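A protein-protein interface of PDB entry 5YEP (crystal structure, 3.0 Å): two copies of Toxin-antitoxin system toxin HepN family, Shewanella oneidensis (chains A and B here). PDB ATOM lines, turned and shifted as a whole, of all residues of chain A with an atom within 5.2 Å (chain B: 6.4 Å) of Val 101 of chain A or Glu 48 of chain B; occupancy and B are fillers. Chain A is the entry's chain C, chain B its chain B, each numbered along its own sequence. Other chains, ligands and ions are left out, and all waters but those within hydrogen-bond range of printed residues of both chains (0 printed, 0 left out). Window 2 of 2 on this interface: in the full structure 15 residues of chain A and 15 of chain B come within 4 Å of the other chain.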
ATOM      1  N   GLN A  44      24.613 -26.637  18.258  1.00  0.00           N
ATOM      2  CA  GLN A  44      23.636 -27.697  18.471  1.00  0.00           C
ATOM      3  C   GLN A  44      23.336 -28.440  17.176  1.00  0.00           C
ATOM      4  O   GLN A  44      23.172 -29.666  17.180  1.00  0.00           O
ATOM      5  CB  GLN A  44      22.356 -27.107  19.060  1.00  0.00           C
ATOM      6  CG  GLN A  44      21.223 -28.097  19.229  1.00  0.00           C
ATOM      7  CD  GLN A  44      19.936 -27.425  19.652  1.00  0.00           C
ATOM      8  OE1 GLN A  44      19.909 -26.221  19.906  1.00  0.00           O
ATOM      9  NE2 GLN A  44      18.859 -28.198  19.722  1.00  0.00           N
ATOM     10  N   GLU A  48      23.585 -32.594  16.517  1.00  0.00           N
ATOM     11  CA  GLU A  48      22.506 -33.435  16.017  1.00  0.00           C
ATOM     12  C   GLU A  48      22.758 -33.924  14.600  1.00  0.00           C
ATOM     13  O   GLU A  48      22.171 -34.932  14.195  1.00  0.00           O
ATOM     14  CB  GLU A  48      21.180 -32.683  16.084  1.00  0.00           C
ATOM     15  CG  GLU A  48      20.500 -32.778  17.434  1.00  0.00           C
ATOM     16  CD  GLU A  48      20.044 -31.432  17.940  1.00  0.00           C
ATOM     17  OE1 GLU A  48      19.350 -31.382  18.977  1.00  0.00           O
ATOM     18  OE2 GLU A  48      20.390 -30.421  17.295  1.00  0.00           O
ATOM     19  N   ARG A  97      25.376 -29.901  24.172  1.00  0.00           N
ATOM     20  CA  ARG A  97      24.110 -29.869  23.448  1.00  0.00           C
ATOM     21  C   ARG A  97      22.925 -30.158  24.365  1.00  0.00           C
ATOM     22  O   ARG A  97      21.850 -29.575  24.184  1.00  0.00           O
ATOM     23  CB  ARG A  97      24.160 -30.862  22.283  1.00  0.00           C
ATOM     24  CG  ARG A  97      22.831 -31.110  21.582  1.00  0.00           C
ATOM     25  CD  ARG A  97      22.268 -32.476  21.948  1.00  0.00           C
ATOM     26  NE  ARG A  97      21.284 -32.950  20.980  1.00  0.00           N
ATOM     27  CZ  ARG A  97      20.748 -34.166  21.000  1.00  0.00           C
ATOM     28  NH1 ARG A  97      21.108 -35.034  21.935  1.00  0.00           N
ATOM     29  NH2 ARG A  97      19.858 -34.519  20.082  1.00  0.00           N
ATOM     30  N   ASN A  98      23.100 -31.037  25.355  1.00  0.00           N
ATOM     31  CA  ASN A  98      22.000 -31.355  26.262  1.00  0.00           C
ATOM     32  C   ASN A  98      21.664 -30.192  27.185  1.00  0.00           C
ATOM     33  O   ASN A  98      20.490 -29.989  27.513  1.00  0.00           O
ATOM     34  CB  ASN A  98      22.330 -32.601  27.082  1.00  0.00           C
ATOM     35  CG  ASN A  98      22.283 -33.873  26.256  1.00  0.00           C
ATOM     36  OD1 ASN A  98      21.681 -33.906  25.181  1.00  0.00           O
ATOM     37  ND2 ASN A  98      22.915 -34.930  26.755  1.00  0.00           N
ATOM     38  N   ILE A  99      22.667 -29.421  27.615  1.00  0.00           N
ATOM     39  CA  ILE A  99      22.398 -28.274  28.480  1.00  0.00           C
ATOM     40  C   ILE A  99      21.668 -27.180  27.713  1.00  0.00           C
ATOM     41  O   ILE A  99      20.832 -26.465  28.281  1.00  0.00           O
ATOM     42  CB  ILE A  99      23.708 -27.745  29.097  1.00  0.00           C
ATOM     43  CG1 ILE A  99      24.506 -28.876  29.752  1.00  0.00           C
ATOM     44  CG2 ILE A  99      23.423 -26.644  30.115  1.00  0.00           C
ATOM     45  CD1 ILE A  99      24.054 -29.231  31.151  1.00  0.00           C
ATOM     46  N   ALA A 100      21.965 -27.025  26.421  1.00  0.00           N
ATOM     47  CA  ALA A 100      21.300 -25.993  25.630  1.00  0.00           C
ATOM     48  C   ALA A 100      19.849 -26.356  25.351  1.00  0.00           C
ATOM     49  O   ALA A 100      18.962 -25.497  25.430  1.00  0.00           O
ATOM     50  CB  ALA A 100      22.052 -25.765  24.320  1.00  0.00           C
ATOM     51  N   VAL A 101      19.592 -27.615  25.010  1.00  0.00           N
ATOM     52  CA  VAL A 101      18.233 -28.079  24.726  1.00  0.00           C
ATOM     53  C   VAL A 101      17.405 -28.234  25.971  1.00  0.00           C
ATOM     54  O   VAL A 101      16.327 -27.643  26.092  1.00  0.00           O
ATOM     55  CB  VAL A 101      18.254 -29.433  23.985  1.00  0.00           C
ATOM     56  CG1 VAL A 101      16.843 -29.889  23.680  1.00  0.00           C
ATOM     57  CG2 VAL A 101      19.057 -29.344  22.706  1.00  0.00           C
ATOM     58  N   HIS A 102      17.891 -29.044  26.906  1.00  0.00           N
ATOM     59  CA  HIS A 102      17.183 -29.284  28.169  1.00  0.00           C
ATOM     60  C   HIS A 102      17.883 -28.439  29.218  1.00  0.00           C
ATOM     61  O   HIS A 102      19.115 -28.383  29.283  1.00  0.00           O
ATOM     62  CB  HIS A 102      17.199 -30.754  28.553  1.00  0.00           C
ATOM     63  CG  HIS A 102      16.813 -31.679  27.440  1.00  0.00           C
ATOM     64  ND1 HIS A 102      17.740 -32.268  26.607  1.00  0.00           N
ATOM     65  CD2 HIS A 102      15.601 -32.102  27.013  1.00  0.00           C
ATOM     66  CE1 HIS A 102      17.115 -33.027  25.724  1.00  0.00           C
ATOM     67  NE2 HIS A 102      15.816 -32.942  25.947  1.00  0.00           N
ATOM     68  N   ASP A 103      17.084 -27.787  30.053  1.00  0.00           N
ATOM     69  CA  ASP A 103      17.580 -26.749  30.953  1.00  0.00           C
ATOM     70  C   ASP A 103      17.820 -27.464  32.283  1.00  0.00           C
ATOM     71  O   ASP A 103      17.060 -27.298  33.235  1.00  0.00           O
ATOM     72  CB  ASP A 103      16.519 -25.664  31.094  1.00  0.00           C
ATOM     73  CG  ASP A 103      17.079 -24.365  31.621  1.00  0.00           C
ATOM     74  OD1 ASP A 103      18.316 -24.267  31.762  1.00  0.00           O
ATOM     75  OD2 ASP A 103      16.283 -23.444  31.902  1.00  0.00           O
ATOM     76  N   LYS B   8       9.984 -22.210  34.619  1.00  0.00           N
ATOM     77  CA  LYS B   8       9.729 -22.425  33.198  1.00  0.00           C
ATOM     78  C   LYS B   8       8.862 -21.314  32.617  1.00  0.00           C
ATOM     79  O   LYS B   8       9.100 -20.862  31.492  1.00  0.00           O
ATOM     80  CB  LYS B   8       9.076 -23.790  32.981  1.00  0.00           C
ATOM     81  CG  LYS B   8      10.004 -24.966  33.240  1.00  0.00           C
ATOM     82  CD  LYS B   8      11.152 -24.981  32.245  1.00  0.00           C
ATOM     83  CE  LYS B   8      12.097 -26.143  32.501  1.00  0.00           C
ATOM     84  NZ  LYS B   8      13.249 -26.127  31.558  1.00  0.00           N
ATOM     85  N   LEU B  43      12.541 -19.792  20.180  1.00  0.00           N
ATOM     86  CA  LEU B  43      11.350 -20.581  19.887  1.00  0.00           C
ATOM     87  C   LEU B  43      11.497 -22.000  20.418  1.00  0.00           C
ATOM     88  O   LEU B  43      10.531 -22.590  20.916  1.00  0.00           O
ATOM     89  CB  LEU B  43      11.083 -20.597  18.381  1.00  0.00           C
ATOM     90  CG  LEU B  43      10.324 -19.404  17.800  1.00  0.00           C
ATOM     91  CD1 LEU B  43      10.331 -19.457  16.281  1.00  0.00           C
ATOM     92  CD2 LEU B  43       8.897 -19.373  18.332  1.00  0.00           C
ATOM     93  N   GLN B  44      12.702 -22.563  20.319  1.00  0.00           N
ATOM     94  CA  GLN B  44      12.965 -23.871  20.911  1.00  0.00           C
ATOM     95  C   GLN B  44      12.923 -23.798  22.433  1.00  0.00           C
ATOM     96  O   GLN B  44      12.315 -24.652  23.088  1.00  0.00           O
ATOM     97  CB  GLN B  44      14.318 -24.398  20.432  1.00  0.00           C
ATOM     98  CG  GLN B  44      15.002 -25.340  21.406  1.00  0.00           C
ATOM     99  CD  GLN B  44      16.294 -25.914  20.855  1.00  0.00           C
ATOM    100  OE1 GLN B  44      16.311 -26.515  19.783  1.00  0.00           O
ATOM    101  NE2 GLN B  44      17.385 -25.732  21.591  1.00  0.00           N
ATOM    102  N   ARG B  45      13.566 -22.779  23.011  1.00  0.00           N
ATOM    103  CA  ARG B  45      13.539 -22.614  24.462  1.00  0.00           C
ATOM    104  C   ARG B  45      12.112 -22.445  24.970  1.00  0.00           C
ATOM    105  O   ARG B  45      11.758 -22.966  26.034  1.00  0.00           O
ATOM    106  CB  ARG B  45      14.398 -21.420  24.873  1.00  0.00           C
ATOM    107  CG  ARG B  45      15.890 -21.634  24.708  1.00  0.00           C
ATOM    108  CD  ARG B  45      16.641 -20.343  24.973  1.00  0.00           C
ATOM    109  NE  ARG B  45      18.084 -20.495  24.824  1.00  0.00           N
ATOM    110  CZ  ARG B  45      18.937 -19.478  24.794  1.00  0.00           C
ATOM    111  NH1 ARG B  45      18.488 -18.235  24.903  1.00  0.00           N
ATOM    112  NH2 ARG B  45      20.237 -19.701  24.656  1.00  0.00           N
ATOM    113  N   CYS B  46      11.279 -21.716  24.222  1.00  0.00           N
ATOM    114  CA  CYS B  46       9.862 -21.638  24.559  1.00  0.00           C
ATOM    115  C   CYS B  46       9.187 -22.995  24.405  1.00  0.00           C
ATOM    116  O   CYS B  46       8.396 -23.404  25.264  1.00  0.00           O
ATOM    117  CB  CYS B  46       9.164 -20.601  23.681  1.00  0.00           C
ATOM    118  SG  CYS B  46       9.374 -18.890  24.212  1.00  0.00           S
ATOM    119  N   CYS B  47       9.490 -23.706  23.319  1.00  0.00           N
ATOM    120  CA  CYS B  47       8.843 -24.990  23.066  1.00  0.00           C
ATOM    121  C   CYS B  47       9.255 -26.033  24.098  1.00  0.00           C
ATOM    122  O   CYS B  47       8.406 -26.768  24.617  1.00  0.00           O
ATOM    123  CB  CYS B  47       9.177 -25.471  21.653  1.00  0.00           C
ATOM    124  SG  CYS B  47       8.173 -26.851  21.069  1.00  0.00           S
ATOM    125  N   GLU B  48      10.550 -26.108  24.412  1.00  0.00           N
ATOM    126  CA  GLU B  48      11.024 -27.128  25.342  1.00  0.00           C
ATOM    127  C   GLU B  48      10.476 -26.898  26.744  1.00  0.00           C
ATOM    128  O   GLU B  48      10.130 -27.857  27.444  1.00  0.00           O
ATOM    129  CB  GLU B  48      12.551 -27.156  25.360  1.00  0.00           C
ATOM    130  CG  GLU B  48      13.167 -27.828  24.146  1.00  0.00           C
ATOM    131  CD  GLU B  48      12.823 -29.305  24.051  1.00  0.00           C
ATOM    132  OE1 GLU B  48      12.848 -29.845  22.926  1.00  0.00           O
ATOM    133  OE2 GLU B  48      12.540 -29.927  25.097  1.00  0.00           O
ATOM    134  N   ALA B  49      10.389 -25.637  27.173  1.00  0.00           N
ATOM    135  CA  ALA B  49       9.847 -25.352  28.496  1.00  0.00           C
ATOM    136  C   ALA B  49       8.396 -25.804  28.604  1.00  0.00           C
ATOM    137  O   ALA B  49       7.976 -26.327  29.642  1.00  0.00           O
ATOM    138  CB  ALA B  49       9.977 -23.863  28.809  1.00  0.00           C
ATOM    139  N   CYS B  50       7.615 -25.621  27.536  1.00  0.00           N
ATOM    140  CA  CYS B  50       6.244 -26.119  27.536  1.00  0.00           C
ATOM    141  C   CYS B  50       6.211 -27.642  27.576  1.00  0.00           C
ATOM    142  O   CYS B  50       5.352 -28.232  28.243  1.00  0.00           O
ATOM    143  CB  CYS B  50       5.490 -25.593  26.314  1.00  0.00           C
ATOM    144  SG  CYS B  50       5.255 -23.798  26.293  1.00  0.00           S
ATOM    145  N   ILE B  51       7.134 -28.296  26.868  1.00  0.00           N
ATOM    146  CA  ILE B  51       7.240 -29.750  26.942  1.00  0.00           C
ATOM    147  C   ILE B  51       7.634 -30.177  28.350  1.00  0.00           C
ATOM    148  O   ILE B  51       7.141 -31.184  28.875  1.00  0.00           O
ATOM    149  CB  ILE B  51       8.240 -30.264  25.889  1.00  0.00           C
ATOM    150  CG1 ILE B  51       7.697 -30.018  24.481  1.00  0.00           C
ATOM    151  CG2 ILE B  51       8.543 -31.744  26.098  1.00  0.00           C
ATOM    152  CD1 ILE B  51       8.617 -30.495  23.382  1.00  0.00           C
ATOM    153  N   ASP B  52       8.523 -29.409  28.988  1.00  0.00           N
ATOM    154  CA  ASP B  52       8.904 -29.699  30.366  1.00  0.00           C
ATOM    155  C   ASP B  52       7.730 -29.489  31.316  1.00  0.00           C
ATOM    156  O   ASP B  52       7.537 -30.270  32.256  1.00  0.00           O
ATOM    157  CB  ASP B  52      10.095 -28.828  30.774  1.00  0.00           C
ATOM    158  CG  ASP B  52      11.339 -29.101  29.937  1.00  0.00           C
ATOM    159  OD1 ASP B  52      11.434 -30.191  29.334  1.00  0.00           O
ATOM    160  OD2 ASP B  52      12.225 -28.219  29.880  1.00  0.00           O
ATOM    161  N   ILE B  53       6.934 -28.441  31.087  1.00  0.00           N
ATOM    162  CA  ILE B  53       5.742 -28.216  31.902  1.00  0.00           C
ATOM    163  C   ILE B  53       4.739 -29.342  31.694  1.00  0.00           C
ATOM    164  O   ILE B  53       4.130 -29.839  32.651  1.00  0.00           O
ATOM    165  CB  ILE B  53       5.125 -26.843  31.576  1.00  0.00           C
ATOM    166  CG1 ILE B  53       6.025 -25.718  32.094  1.00  0.00           C
ATOM    167  CG2 ILE B  53       3.724 -26.727  32.163  1.00  0.00           C
ATOM    168  CD1 ILE B  53       5.547 -24.329  31.726  1.00  0.00           C
ATOM    169  N   SER B  69       7.054 -36.241  22.738  1.00  0.00           N
ATOM    170  CA  SER B  69       6.863 -34.863  23.170  1.00  0.00           C
ATOM    171  C   SER B  69       5.438 -34.399  22.897  1.00  0.00           C
ATOM    172  O   SER B  69       4.853 -33.663  23.700  1.00  0.00           O
ATOM    173  CB  SER B  69       7.875 -33.951  22.479  1.00  0.00           C
ATOM    174  OG  SER B  69       9.176 -34.513  22.519  1.00  0.00           O
ATOM    175  N   VAL B  94       6.318 -28.107  17.968  1.00  0.00           N
ATOM    176  CA  VAL B  94       7.380 -29.111  18.014  1.00  0.00           C
ATOM    177  C   VAL B  94       7.773 -29.533  16.601  1.00  0.00           C
ATOM    178  O   VAL B  94       8.951 -29.779  16.314  1.00  0.00           O
ATOM    179  CB  VAL B  94       6.942 -30.315  18.872  1.00  0.00           C
ATOM    180  CG1 VAL B  94       8.111 -31.267  19.091  1.00  0.00           C
ATOM    181  CG2 VAL B  94       6.388 -29.827  20.204  1.00  0.00           C
ATOM    182  N   ARG B  97       9.855 -26.826  15.469  1.00  0.00           N
ATOM    183  CA  ARG B  97      11.132 -26.906  16.171  1.00  0.00           C
ATOM    184  C   ARG B  97      12.049 -27.932  15.517  1.00  0.00           C
ATOM    185  O   ARG B  97      13.184 -27.620  15.139  1.00  0.00           O
ATOM    186  CB  ARG B  97      10.907 -27.254  17.641  1.00  0.00           C
ATOM    187  CG  ARG B  97      12.184 -27.242  18.460  1.00  0.00           C
ATOM    188  CD  ARG B  97      12.153 -28.295  19.552  1.00  0.00           C
ATOM    189  NE  ARG B  97      12.858 -29.513  19.160  1.00  0.00           N
ATOM    190  CZ  ARG B  97      14.122 -29.778  19.477  1.00  0.00           C
ATOM    191  NH1 ARG B  97      14.822 -28.910  20.194  1.00  0.00           N
ATOM    192  NH2 ARG B  97      14.687 -30.910  19.081  1.00  0.00           N
ATOM    193  N   ASN B  98      11.566 -29.170  15.374  1.00  0.00           N
ATOM    194  CA  ASN B  98      12.392 -30.237  14.818  1.00  0.00           C
ATOM    195  C   ASN B  98      12.864 -29.897  13.411  1.00  0.00           C
ATOM    196  O   ASN B  98      14.034 -30.115  13.071  1.00  0.00           O
ATOM    197  CB  ASN B  98      11.612 -31.551  14.810  1.00  0.00           C
ATOM    198  CG  ASN B  98      11.232 -32.014  16.201  1.00  0.00           C
ATOM    199  OD1 ASN B  98      11.832 -31.596  17.191  1.00  0.00           O
ATOM    200  ND2 ASN B  98      10.230 -32.881  16.282  1.00  0.00           N
ATOM    201  N   VAL B 101      15.833 -27.235  13.819  1.00  0.00           N
ATOM    202  CA  VAL B 101      17.094 -27.624  14.441  1.00  0.00           C
ATOM    203  C   VAL B 101      17.882 -28.653  13.639  1.00  0.00           C
ATOM    204  O   VAL B 101      19.051 -28.431  13.307  1.00  0.00           O
ATOM    205  CB  VAL B 101      16.861 -28.221  15.838  1.00  0.00           C
ATOM    206  CG1 VAL B 101      18.172 -28.348  16.562  1.00  0.00           C
ATOM    207  CG2 VAL B 101      15.911 -27.348  16.634  1.00  0.00           C
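Of the printed residues of chain B, Val 101 of chain A touches Glu 48.
Printed residues of chain B within 4 Å of Gln 44 of chain A: Gln 44 and Val 101.
Printed residues of chain A within 4 Å of Val 101 of chain B: Gln 44 and Glu 48.
The nearest printed residue of chain A that does not touch Val 101 of chain B is Val 101 of chain A (6.3 Å).
The side-chain amino group (NZ) of Lys 8 of chain B is in salt-bridge range of the side-chain carboxylate (OD2) of Asp 52 of chain B, at 2.9 Å.
The side-chain amide oxygen (OE1) of Gln 44 of chain B is in hydrogen-bond range of the guanidinium group (NH1) of Arg 97 of chain B (2.8 Å).
The guanidinium group (NH1) of Arg 97 of chain B is in salt-bridge range of the side-chain carboxylate (OE1) of Glu 48 of chain B (3.5 Å).
The side-chain amide nitrogen (NE2) of Gln 44 of chain A is in hydrogen-bond range of the side-chain carboxylate (OE1) of Glu 48 of chain A, at 3.3 Å.
The guanidinium group of Arg 97 of chain A lies within salt-bridge range of the side-chain carboxylate of Glu 48 of chain A, 3.2 Å away.
Along chain A the printed residues that touch a printed residue of chain B span positions 44 to 103.
Of the 17 printed residues of chain B, 4 touch a printed residue of chain A.
Printed residues of chain B that touch a printed residue of chain A: Lys 8, Gln 44, Glu 48 and Val 101.
Along chain B the printed residues that touch a printed residue of chain A span positions 8 to 101.
The side-chain amide oxygen (OE1) of Gln 44 of chain B lies within hydrogen-bond range of the side-chain amide nitrogen (NE2) of Gln 44 of chain A.
Gln 44 of chain A touches its own counterpart, Gln 44 of chain B.
Gln 44 of chain A touches Val 101 of chain B, but with the chains exchanged Val 101 of chain A does not touch Gln 44 of chain B (4.01 Å).
Glu 48 of chain A touches Val 101 of chain B, and with the chains exchanged Val 101 of chain A touches Glu 48 of chain B.
Positions printed for both chains: 44, 48, 97, 98 and 101.
Of the 5 pairs that touch across the chains among the printed residues, 3 have their exchanged pair printed and touching as well.
Among the printed residues, merely in contact across the chains: Glu 48 of chain A with Val 101 of chain B (3.1 Å), Gln 44 of chain A with Val 101 of chain B (3.2 Å), Asp 103 of chain A with Lys 8 of chain B (3.3 Å) and Val 101 of chain A with Glu 48 of chain B (3.7 Å).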
